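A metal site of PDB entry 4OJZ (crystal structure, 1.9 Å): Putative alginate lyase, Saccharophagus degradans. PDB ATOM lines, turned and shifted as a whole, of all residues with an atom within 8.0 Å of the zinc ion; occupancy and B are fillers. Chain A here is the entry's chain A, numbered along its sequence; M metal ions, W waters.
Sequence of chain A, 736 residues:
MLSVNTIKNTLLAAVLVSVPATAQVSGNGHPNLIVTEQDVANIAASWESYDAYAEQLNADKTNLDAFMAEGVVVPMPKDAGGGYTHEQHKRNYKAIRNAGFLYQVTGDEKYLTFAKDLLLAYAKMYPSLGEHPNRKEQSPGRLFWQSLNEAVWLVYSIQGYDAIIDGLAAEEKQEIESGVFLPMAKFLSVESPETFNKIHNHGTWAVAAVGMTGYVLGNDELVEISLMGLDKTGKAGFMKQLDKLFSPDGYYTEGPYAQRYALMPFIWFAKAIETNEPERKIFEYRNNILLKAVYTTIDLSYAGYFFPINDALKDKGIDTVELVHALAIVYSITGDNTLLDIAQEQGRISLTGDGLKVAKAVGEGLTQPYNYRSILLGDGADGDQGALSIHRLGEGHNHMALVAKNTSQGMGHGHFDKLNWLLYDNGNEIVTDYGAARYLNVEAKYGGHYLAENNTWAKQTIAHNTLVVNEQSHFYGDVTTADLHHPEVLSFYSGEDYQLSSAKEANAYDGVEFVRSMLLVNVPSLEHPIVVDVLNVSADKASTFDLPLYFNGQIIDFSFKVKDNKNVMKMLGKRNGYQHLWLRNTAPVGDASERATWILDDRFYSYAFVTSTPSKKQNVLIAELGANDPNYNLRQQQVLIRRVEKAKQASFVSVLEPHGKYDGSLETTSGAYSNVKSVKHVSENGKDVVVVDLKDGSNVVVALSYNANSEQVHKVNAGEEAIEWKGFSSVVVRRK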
ATOM      1  N   PRO A 308     -13.960  -8.627  -3.225  1.00  0.00           N
ATOM      2  CA  PRO A 308     -14.139  -7.446  -2.367  1.00  0.00           C
ATOM      3  C   PRO A 308     -15.061  -6.400  -2.967  1.00  0.00           C
ATOM      4  O   PRO A 308     -14.673  -5.228  -3.090  1.00  0.00           O
ATOM      5  CB  PRO A 308     -12.710  -6.914  -2.224  1.00  0.00           C
ATOM      6  CG  PRO A 308     -12.054  -7.303  -3.499  1.00  0.00           C
ATOM      7  CD  PRO A 308     -12.623  -8.652  -3.844  1.00  0.00           C
ATOM      8  N   ILE A 309     -16.276  -6.798  -3.304  1.00  0.00           N
ATOM      9  CA  ILE A 309     -17.266  -5.876  -3.854  1.00  0.00           C
ATOM     10  C   ILE A 309     -18.044  -5.164  -2.758  1.00  0.00           C
ATOM     11  O   ILE A 309     -18.223  -5.695  -1.656  1.00  0.00           O
ATOM     12  CB  ILE A 309     -18.213  -6.545  -4.860  1.00  0.00           C
ATOM     13  CG1 ILE A 309     -18.990  -7.706  -4.214  1.00  0.00           C
ATOM     14  CG2 ILE A 309     -17.419  -7.008  -6.083  1.00  0.00           C
ATOM     15  CD1 ILE A 309     -20.212  -8.162  -4.983  1.00  0.00           C
ATOM     16  N   ASN A 310     -18.493  -3.940  -3.051  1.00  0.00           N
ATOM     17  CA  ASN A 310     -19.155  -3.099  -2.070  1.00  0.00           C
ATOM     18  C   ASN A 310     -18.286  -2.969  -0.810  1.00  0.00           C
ATOM     19  O   ASN A 310     -17.066  -3.004  -0.882  1.00  0.00           O
ATOM     20  CB  ASN A 310     -20.563  -3.625  -1.738  1.00  0.00           C
ATOM     21  CG  ASN A 310     -21.488  -3.627  -2.957  1.00  0.00           C
ATOM     22  OD1 ASN A 310     -21.428  -2.724  -3.800  1.00  0.00           O
ATOM     23  ND2 ASN A 310     -22.353  -4.625  -3.031  1.00  0.00           N
ATOM     24  N   ASP A 311     -18.931  -2.813   0.344  1.00  0.00           N
ATOM     25  CA  ASP A 311     -18.208  -2.754   1.614  1.00  0.00           C
ATOM     26  C   ASP A 311     -17.539  -4.104   1.836  1.00  0.00           C
ATOM     27  O   ASP A 311     -18.210  -5.126   1.972  1.00  0.00           O
ATOM     28  CB  ASP A 311     -19.187  -2.466   2.748  1.00  0.00           C
ATOM     29  CG  ASP A 311     -18.522  -2.483   4.097  1.00  0.00           C
ATOM     30  OD1 ASP A 311     -17.681  -1.587   4.326  1.00  0.00           O
ATOM     31  OD2 ASP A 311     -18.844  -3.375   4.918  1.00  0.00           O
ATOM     32  N   ALA A 312     -16.212  -4.103   1.845  1.00  0.00           N
ATOM     33  CA  ALA A 312     -15.445  -5.337   1.997  1.00  0.00           C
ATOM     34  C   ALA A 312     -14.041  -5.010   2.473  1.00  0.00           C
ATOM     35  O   ALA A 312     -13.506  -3.953   2.143  1.00  0.00           O
ATOM     36  CB  ALA A 312     -15.381  -6.094   0.688  1.00  0.00           C
ATOM     37  N   LYS A 405     -20.254  -7.277 -12.054  1.00  0.00           N
ATOM     38  CA  LYS A 405     -21.128  -6.763 -11.001  1.00  0.00           C
ATOM     39  C   LYS A 405     -22.287  -5.968 -11.598  1.00  0.00           C
ATOM     40  O   LYS A 405     -22.245  -4.730 -11.664  1.00  0.00           O
ATOM     41  CB  LYS A 405     -20.332  -5.912 -10.012  1.00  0.00           C
ATOM     42  CG  LYS A 405     -21.067  -5.564  -8.729  1.00  0.00           C
ATOM     43  CD  LYS A 405     -20.159  -4.768  -7.806  1.00  0.00           C
ATOM     44  CE  LYS A 405     -20.878  -4.360  -6.534  1.00  0.00           C
ATOM     45  NZ  LYS A 405     -21.829  -3.240  -6.771  1.00  0.00           N
ATOM     46  N   HIS A 413     -24.253  -0.027   2.267  1.00  0.00           N
ATOM     47  CA  HIS A 413     -22.963  -0.693   2.059  1.00  0.00           C
ATOM     48  C   HIS A 413     -22.580  -0.766   0.574  1.00  0.00           C
ATOM     49  O   HIS A 413     -21.462  -1.193   0.247  1.00  0.00           O
ATOM     50  CB  HIS A 413     -22.984  -2.101   2.664  1.00  0.00           C
ATOM     51  CG  HIS A 413     -23.093  -2.129   4.158  1.00  0.00           C
ATOM     52  ND1 HIS A 413     -22.231  -1.426   4.978  1.00  0.00           N
ATOM     53  CD2 HIS A 413     -23.959  -2.771   4.978  1.00  0.00           C
ATOM     54  CE1 HIS A 413     -22.575  -1.639   6.242  1.00  0.00           C
ATOM     55  NE2 HIS A 413     -23.614  -2.443   6.262  1.00  0.00           N
ATOM     56  N   GLY A 414     -23.483  -0.362  -0.303  1.00  0.00           N
ATOM     57  CA  GLY A 414     -23.271  -0.518  -1.745  1.00  0.00           C
ATOM     58  C   GLY A 414     -22.355   0.503  -2.398  1.00  0.00           C
ATOM     59  O   GLY A 414     -22.285   1.644  -1.960  1.00  0.00           O
ATOM     60  N   HIS A 415     -21.665   0.088  -3.444  1.00  0.00           N
ATOM     61  CA  HIS A 415     -20.807   1.013  -4.171  1.00  0.00           C
ATOM     62  C   HIS A 415     -21.479   1.516  -5.444  1.00  0.00           C
ATOM     63  O   HIS A 415     -22.409   0.882  -5.963  1.00  0.00           O
ATOM     64  CB  HIS A 415     -19.413   0.390  -4.419  1.00  0.00           C
ATOM     65  CG  HIS A 415     -18.572   0.311  -3.186  1.00  0.00           C
ATOM     66  ND1 HIS A 415     -17.240  -0.027  -3.212  1.00  0.00           N
ATOM     67  CD2 HIS A 415     -18.862   0.568  -1.888  1.00  0.00           C
ATOM     68  CE1 HIS A 415     -16.753  -0.006  -1.977  1.00  0.00           C
ATOM     69  NE2 HIS A 415     -17.719   0.345  -1.159  1.00  0.00           N
ATOM     70  N   PHE A 416     -21.062   2.684  -5.924  1.00  0.00           N
ATOM     71  CA  PHE A 416     -21.657   3.282  -7.115  1.00  0.00           C
ATOM     72  C   PHE A 416     -20.891   2.811  -8.350  1.00  0.00           C
ATOM     73  O   PHE A 416     -20.193   3.571  -9.014  1.00  0.00           O
ATOM     74  CB  PHE A 416     -21.671   4.818  -6.998  1.00  0.00           C
ATOM     75  CG  PHE A 416     -22.441   5.312  -5.805  1.00  0.00           C
ATOM     76  CD1 PHE A 416     -23.829   5.374  -5.845  1.00  0.00           C
ATOM     77  CD2 PHE A 416     -21.786   5.669  -4.639  1.00  0.00           C
ATOM     78  CE1 PHE A 416     -24.556   5.805  -4.737  1.00  0.00           C
ATOM     79  CE2 PHE A 416     -22.503   6.099  -3.528  1.00  0.00           C
ATOM     80  CZ  PHE A 416     -23.888   6.172  -3.576  1.00  0.00           C
ATOM     81  N   ASP A 417     -21.062   1.519  -8.656  1.00  0.00           N
ATOM     82  CA  ASP A 417     -20.200   0.869  -9.637  1.00  0.00           C
ATOM     83  C   ASP A 417     -20.948  -0.120 -10.518  1.00  0.00           C
ATOM     84  O   ASP A 417     -20.513  -1.261 -10.682  1.00  0.00           O
ATOM     85  CB  ASP A 417     -19.019   0.185  -8.904  1.00  0.00           C
ATOM     86  CG  ASP A 417     -19.464  -0.983  -8.013  1.00  0.00           C
ATOM     87  OD1 ASP A 417     -20.657  -1.070  -7.646  1.00  0.00           O
ATOM     88  OD2 ASP A 417     -18.588  -1.819  -7.677  1.00  0.00           O
ATOM     89  N   ASN A 420     -19.383  -2.882 -13.065  1.00  0.00           N
ATOM     90  CA  ASN A 420     -17.998  -3.052 -12.655  1.00  0.00           C
ATOM     91  C   ASN A 420     -17.558  -4.499 -12.882  1.00  0.00           C
ATOM     92  O   ASN A 420     -18.402  -5.375 -12.970  1.00  0.00           O
ATOM     93  CB  ASN A 420     -17.854  -2.718 -11.171  1.00  0.00           C
ATOM     94  CG  ASN A 420     -16.417  -2.752 -10.697  1.00  0.00           C
ATOM     95  OD1 ASN A 420     -15.504  -2.486 -11.449  1.00  0.00           O
ATOM     96  ND2 ASN A 420     -16.217  -3.085  -9.423  1.00  0.00           N
ATOM     97  N   LEU A 422     -14.171  -7.577 -12.026  1.00  0.00           N
ATOM     98  CA  LEU A 422     -12.946  -7.986 -11.352  1.00  0.00           C
ATOM     99  C   LEU A 422     -12.408  -9.182 -12.138  1.00  0.00           C
ATOM    100  O   LEU A 422     -13.173  -9.920 -12.748  1.00  0.00           O
ATOM    101  CB  LEU A 422     -13.231  -8.432  -9.908  1.00  0.00           C
ATOM    102  CG  LEU A 422     -13.563  -7.452  -8.770  1.00  0.00           C
ATOM    103  CD1 LEU A 422     -14.969  -6.883  -8.888  1.00  0.00           C
ATOM    104  CD2 LEU A 422     -13.414  -8.161  -7.425  1.00  0.00           C
ATOM    105  N   THR A 432      -8.891  -5.118 -10.090  1.00  0.00           N
ATOM    106  CA  THR A 432      -9.234  -5.110  -8.680  1.00  0.00           C
ATOM    107  C   THR A 432     -10.372  -4.168  -8.270  1.00  0.00           C
ATOM    108  O   THR A 432     -10.716  -3.223  -8.995  1.00  0.00           O
ATOM    109  CB  THR A 432      -8.008  -4.803  -7.802  1.00  0.00           C
ATOM    110  OG1 THR A 432      -7.579  -3.442  -8.035  1.00  0.00           O
ATOM    111  CG2 THR A 432      -6.868  -5.752  -8.114  1.00  0.00           C
ATOM    112  N   ASP A 433     -10.919  -4.454  -7.096  1.00  0.00           N
ATOM    113  CA  ASP A 433     -11.918  -3.619  -6.452  1.00  0.00           C
ATOM    114  C   ASP A 433     -11.334  -3.247  -5.086  1.00  0.00           C
ATOM    115  O   ASP A 433     -10.855  -4.123  -4.344  1.00  0.00           O
ATOM    116  CB  ASP A 433     -13.240  -4.392  -6.319  1.00  0.00           C
ATOM    117  CG  ASP A 433     -14.455  -3.488  -6.063  1.00  0.00           C
ATOM    118  OD1 ASP A 433     -14.293  -2.375  -5.513  1.00  0.00           O
ATOM    119  OD2 ASP A 433     -15.584  -3.906  -6.399  1.00  0.00           O
ATOM    120  N   TYR A 434     -11.363  -1.957  -4.766  1.00  0.00           N
ATOM    121  CA  TYR A 434     -10.699  -1.421  -3.583  1.00  0.00           C
ATOM    122  C   TYR A 434     -11.248  -1.958  -2.266  1.00  0.00           C
ATOM    123  O   TYR A 434     -10.502  -2.127  -1.307  1.00  0.00           O
ATOM    124  CB  TYR A 434     -10.788   0.123  -3.573  1.00  0.00           C
ATOM    125  CG  TYR A 434      -9.838   0.773  -2.578  1.00  0.00           C
ATOM    126  CD1 TYR A 434     -10.254   1.110  -1.283  1.00  0.00           C
ATOM    127  CD2 TYR A 434      -8.500   1.009  -2.917  1.00  0.00           C
ATOM    128  CE1 TYR A 434      -9.381   1.685  -0.368  1.00  0.00           C
ATOM    129  CE2 TYR A 434      -7.623   1.585  -2.012  1.00  0.00           C
ATOM    130  CZ  TYR A 434      -8.059   1.914  -0.748  1.00  0.00           C
ATOM    131  OH  TYR A 434      -7.165   2.472   0.141  1.00  0.00           O
ATOM    132  N   GLY A 435     -12.556  -2.213  -2.209  1.00  0.00           N
ATOM    133  CA  GLY A 435     -13.223  -2.525  -0.956  1.00  0.00           C
ATOM    134  C   GLY A 435     -13.449  -1.237  -0.186  1.00  0.00           C
ATOM    135  O   GLY A 435     -13.520  -0.162  -0.777  1.00  0.00           O
ATOM    136  N   ALA A 436     -13.537  -1.344   1.148  1.00  0.00           N
ATOM    137  CA  ALA A 436     -13.837  -0.184   2.009  1.00  0.00           C
ATOM    138  C   ALA A 436     -12.585   0.512   2.514  1.00  0.00           C
ATOM    139  O   ALA A 436     -11.517  -0.106   2.608  1.00  0.00           O
ATOM    140  CB  ALA A 436     -14.701  -0.620   3.181  1.00  0.00           C
ATOM    141  N   TRP A 457     -13.852   8.338  -1.436  1.00  0.00           N
ATOM    142  CA  TRP A 457     -13.082   7.555  -2.388  1.00  0.00           C
ATOM    143  C   TRP A 457     -13.725   6.205  -2.710  1.00  0.00           C
ATOM    144  O   TRP A 457     -14.163   5.976  -3.841  1.00  0.00           O
ATOM    145  CB  TRP A 457     -11.634   7.320  -1.902  1.00  0.00           C
ATOM    146  CG  TRP A 457     -10.941   6.246  -2.713  1.00  0.00           C
ATOM    147  CD1 TRP A 457     -10.599   4.983  -2.294  1.00  0.00           C
ATOM    148  CD2 TRP A 457     -10.561   6.327  -4.101  1.00  0.00           C
ATOM    149  NE1 TRP A 457     -10.019   4.296  -3.329  1.00  0.00           N
ATOM    150  CE2 TRP A 457      -9.981   5.089  -4.439  1.00  0.00           C
ATOM    151  CE3 TRP A 457     -10.649   7.340  -5.073  1.00  0.00           C
ATOM    152  CZ2 TRP A 457      -9.480   4.832  -5.725  1.00  0.00           C
ATOM    153  CZ3 TRP A 457     -10.151   7.072  -6.351  1.00  0.00           C
ATOM    154  CH2 TRP A 457      -9.583   5.822  -6.662  1.00  0.00           C
ATOM    155  N   ALA A 458     -13.774   5.320  -1.710  1.00  0.00           N
ATOM    156  CA  ALA A 458     -14.002   3.893  -1.941  1.00  0.00           C
ATOM    157  C   ALA A 458     -15.326   3.550  -2.613  1.00  0.00           C
ATOM    158  O   ALA A 458     -15.402   2.603  -3.386  1.00  0.00           O
ATOM    159  CB  ALA A 458     -13.842   3.106  -0.629  1.00  0.00           C
ATOM    160  N   LYS A 459     -16.363   4.340  -2.324  1.00  0.00           N
ATOM    161  CA  LYS A 459     -17.703   4.121  -2.895  1.00  0.00           C
ATOM    162  C   LYS A 459     -17.861   4.684  -4.309  1.00  0.00           C
ATOM    163  O   LYS A 459     -18.771   4.276  -5.042  1.00  0.00           O
ATOM    164  CB  LYS A 459     -18.774   4.758  -2.013  1.00  0.00           C
ATOM    165  CG  LYS A 459     -18.992   4.088  -0.666  1.00  0.00           C
ATOM    166  CD  LYS A 459     -20.198   4.710   0.019  1.00  0.00           C
ATOM    167  CE  LYS A 459     -20.494   4.022   1.343  1.00  0.00           C
ATOM    168  NZ  LYS A 459     -21.596   4.723   2.044  1.00  0.00           N
ATOM    169  N   GLN A 460     -17.000   5.624  -4.675  1.00  0.00           N
ATOM    170  CA  GLN A 460     -17.195   6.405  -5.904  1.00  0.00           C
ATOM    171  C   GLN A 460     -16.868   5.625  -7.171  1.00  0.00           C
ATOM    172  O   GLN A 460     -16.033   4.712  -7.162  1.00  0.00           O
ATOM    173  CB  GLN A 460     -16.395   7.714  -5.835  1.00  0.00           C
ATOM    174  CG  GLN A 460     -16.761   8.632  -4.672  1.00  0.00           C
ATOM    175  CD  GLN A 460     -18.217   9.063  -4.680  1.00  0.00           C
ATOM    176  OE1 GLN A 460     -18.754   9.468  -5.709  1.00  0.00           O
ATOM    177  NE2 GLN A 460     -18.869   8.958  -3.526  1.00  0.00           N
ATOM    178  N   ALA A 463     -13.317   5.063  -8.657  1.00  0.00           N
ATOM    179  CA  ALA A 463     -12.475   4.098  -7.933  1.00  0.00           C
ATOM    180  C   ALA A 463     -12.696   2.671  -8.443  1.00  0.00           C
ATOM    181  O   ALA A 463     -12.086   1.733  -7.944  1.00  0.00           O
ATOM    182  CB  ALA A 463     -12.751   4.160  -6.448  1.00  0.00           C
ATOM    183  N   HIS A 464     -13.578   2.532  -9.438  1.00  0.00           N
ATOM    184  CA  HIS A 464     -13.932   1.218  -9.984  1.00  0.00           C
ATOM    185  C   HIS A 464     -13.638   1.085 -11.467  1.00  0.00           C
ATOM    186  O   HIS A 464     -13.388   2.078 -12.159  1.00  0.00           O
ATOM    187  CB  HIS A 464     -15.417   0.937  -9.709  1.00  0.00           C
ATOM    188  CG  HIS A 464     -15.734   0.840  -8.242  1.00  0.00           C
ATOM    189  ND1 HIS A 464     -15.902   1.955  -7.439  1.00  0.00           N
ATOM    190  CD2 HIS A 464     -15.872  -0.231  -7.433  1.00  0.00           C
ATOM    191  CE1 HIS A 464     -16.144   1.564  -6.200  1.00  0.00           C
ATOM    192  NE2 HIS A 464     -16.139   0.239  -6.175  1.00  0.00           N
ATOM    193  N   ASN A 465     -13.688  -0.152 -11.958  1.00  0.00           N
ATOM    194  CA  ASN A 465     -13.463  -0.471 -13.363  1.00  0.00           C
ATOM    195  C   ASN A 465     -14.742  -0.392 -14.192  1.00  0.00           C
ATOM    196  O   ASN A 465     -15.162  -1.379 -14.818  1.00  0.00           O
ATOM    197  CB  ASN A 465     -12.839  -1.878 -13.456  1.00  0.00           C
ATOM    198  CG  ASN A 465     -11.701  -2.069 -12.477  1.00  0.00           C
ATOM    199  OD1 ASN A 465     -10.754  -1.287 -12.461  1.00  0.00           O
ATOM    200  ND2 ASN A 465     -11.789  -3.111 -11.656  1.00  0.00           N
HETATM  201 ZN    ZN M   1     -15.950  -1.190  -4.584  1.00  0.00          ZN
HETATM  202  O   HOH W   1     -14.400  -0.037  -3.879  1.00  0.00           O
HETATM  203  O   HOH W   2     -15.574  -2.618  -3.002  1.00  0.00           O
HETATM  204  O   HOH W   3     -17.714  -2.461  -5.463  1.00  0.00           O
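OD1 of Asn 310 lies within hydrogen-bond range of N of His 415 (2.8 Å). OD2 of Asp 433 lies within hydrogen-bond range of ND2 of Asn 420 (3.2 Å). ND1 of His 464 is in hydrogen-bond range of O of Gln 460, 2.8 Å away. A ring nitrogen (ND1) of His 415 sits close to the backbone carbonyl oxygen (O) of Ala 458, at 3.2 Å.
Along chain A the residues within 4 Å of the zinc ion span positions 415 to 464. The nearest printed residue that does not touch the zinc ion is Ala 458 (4.02 Å).
The zinc ion is bound by water W1 (2.1 Å), a ring nitrogen (NE2) of His 464 (2.1 Å), water W2 (2.2 Å), a ring nitrogen (ND1) of His 415 (2.2 Å), the side-chain carboxylate of Asp 433 (2.2 Å) and water W3 (2.3 Å).
Water W2 lies within hydrogen-bond range of O of Asn 310 (2.6 Å), O of Pro 308 (2.8 Å) and N of Gly 435 (3.1 Å). Water W1 bridges O of Ala 458 (2.9 Å) and O of Gly 435 (3.2 Å). Water W3 lies within hydrogen-bond range of OD2 of Asp 417, OD2 of Asp 433 and N of Asn 310.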
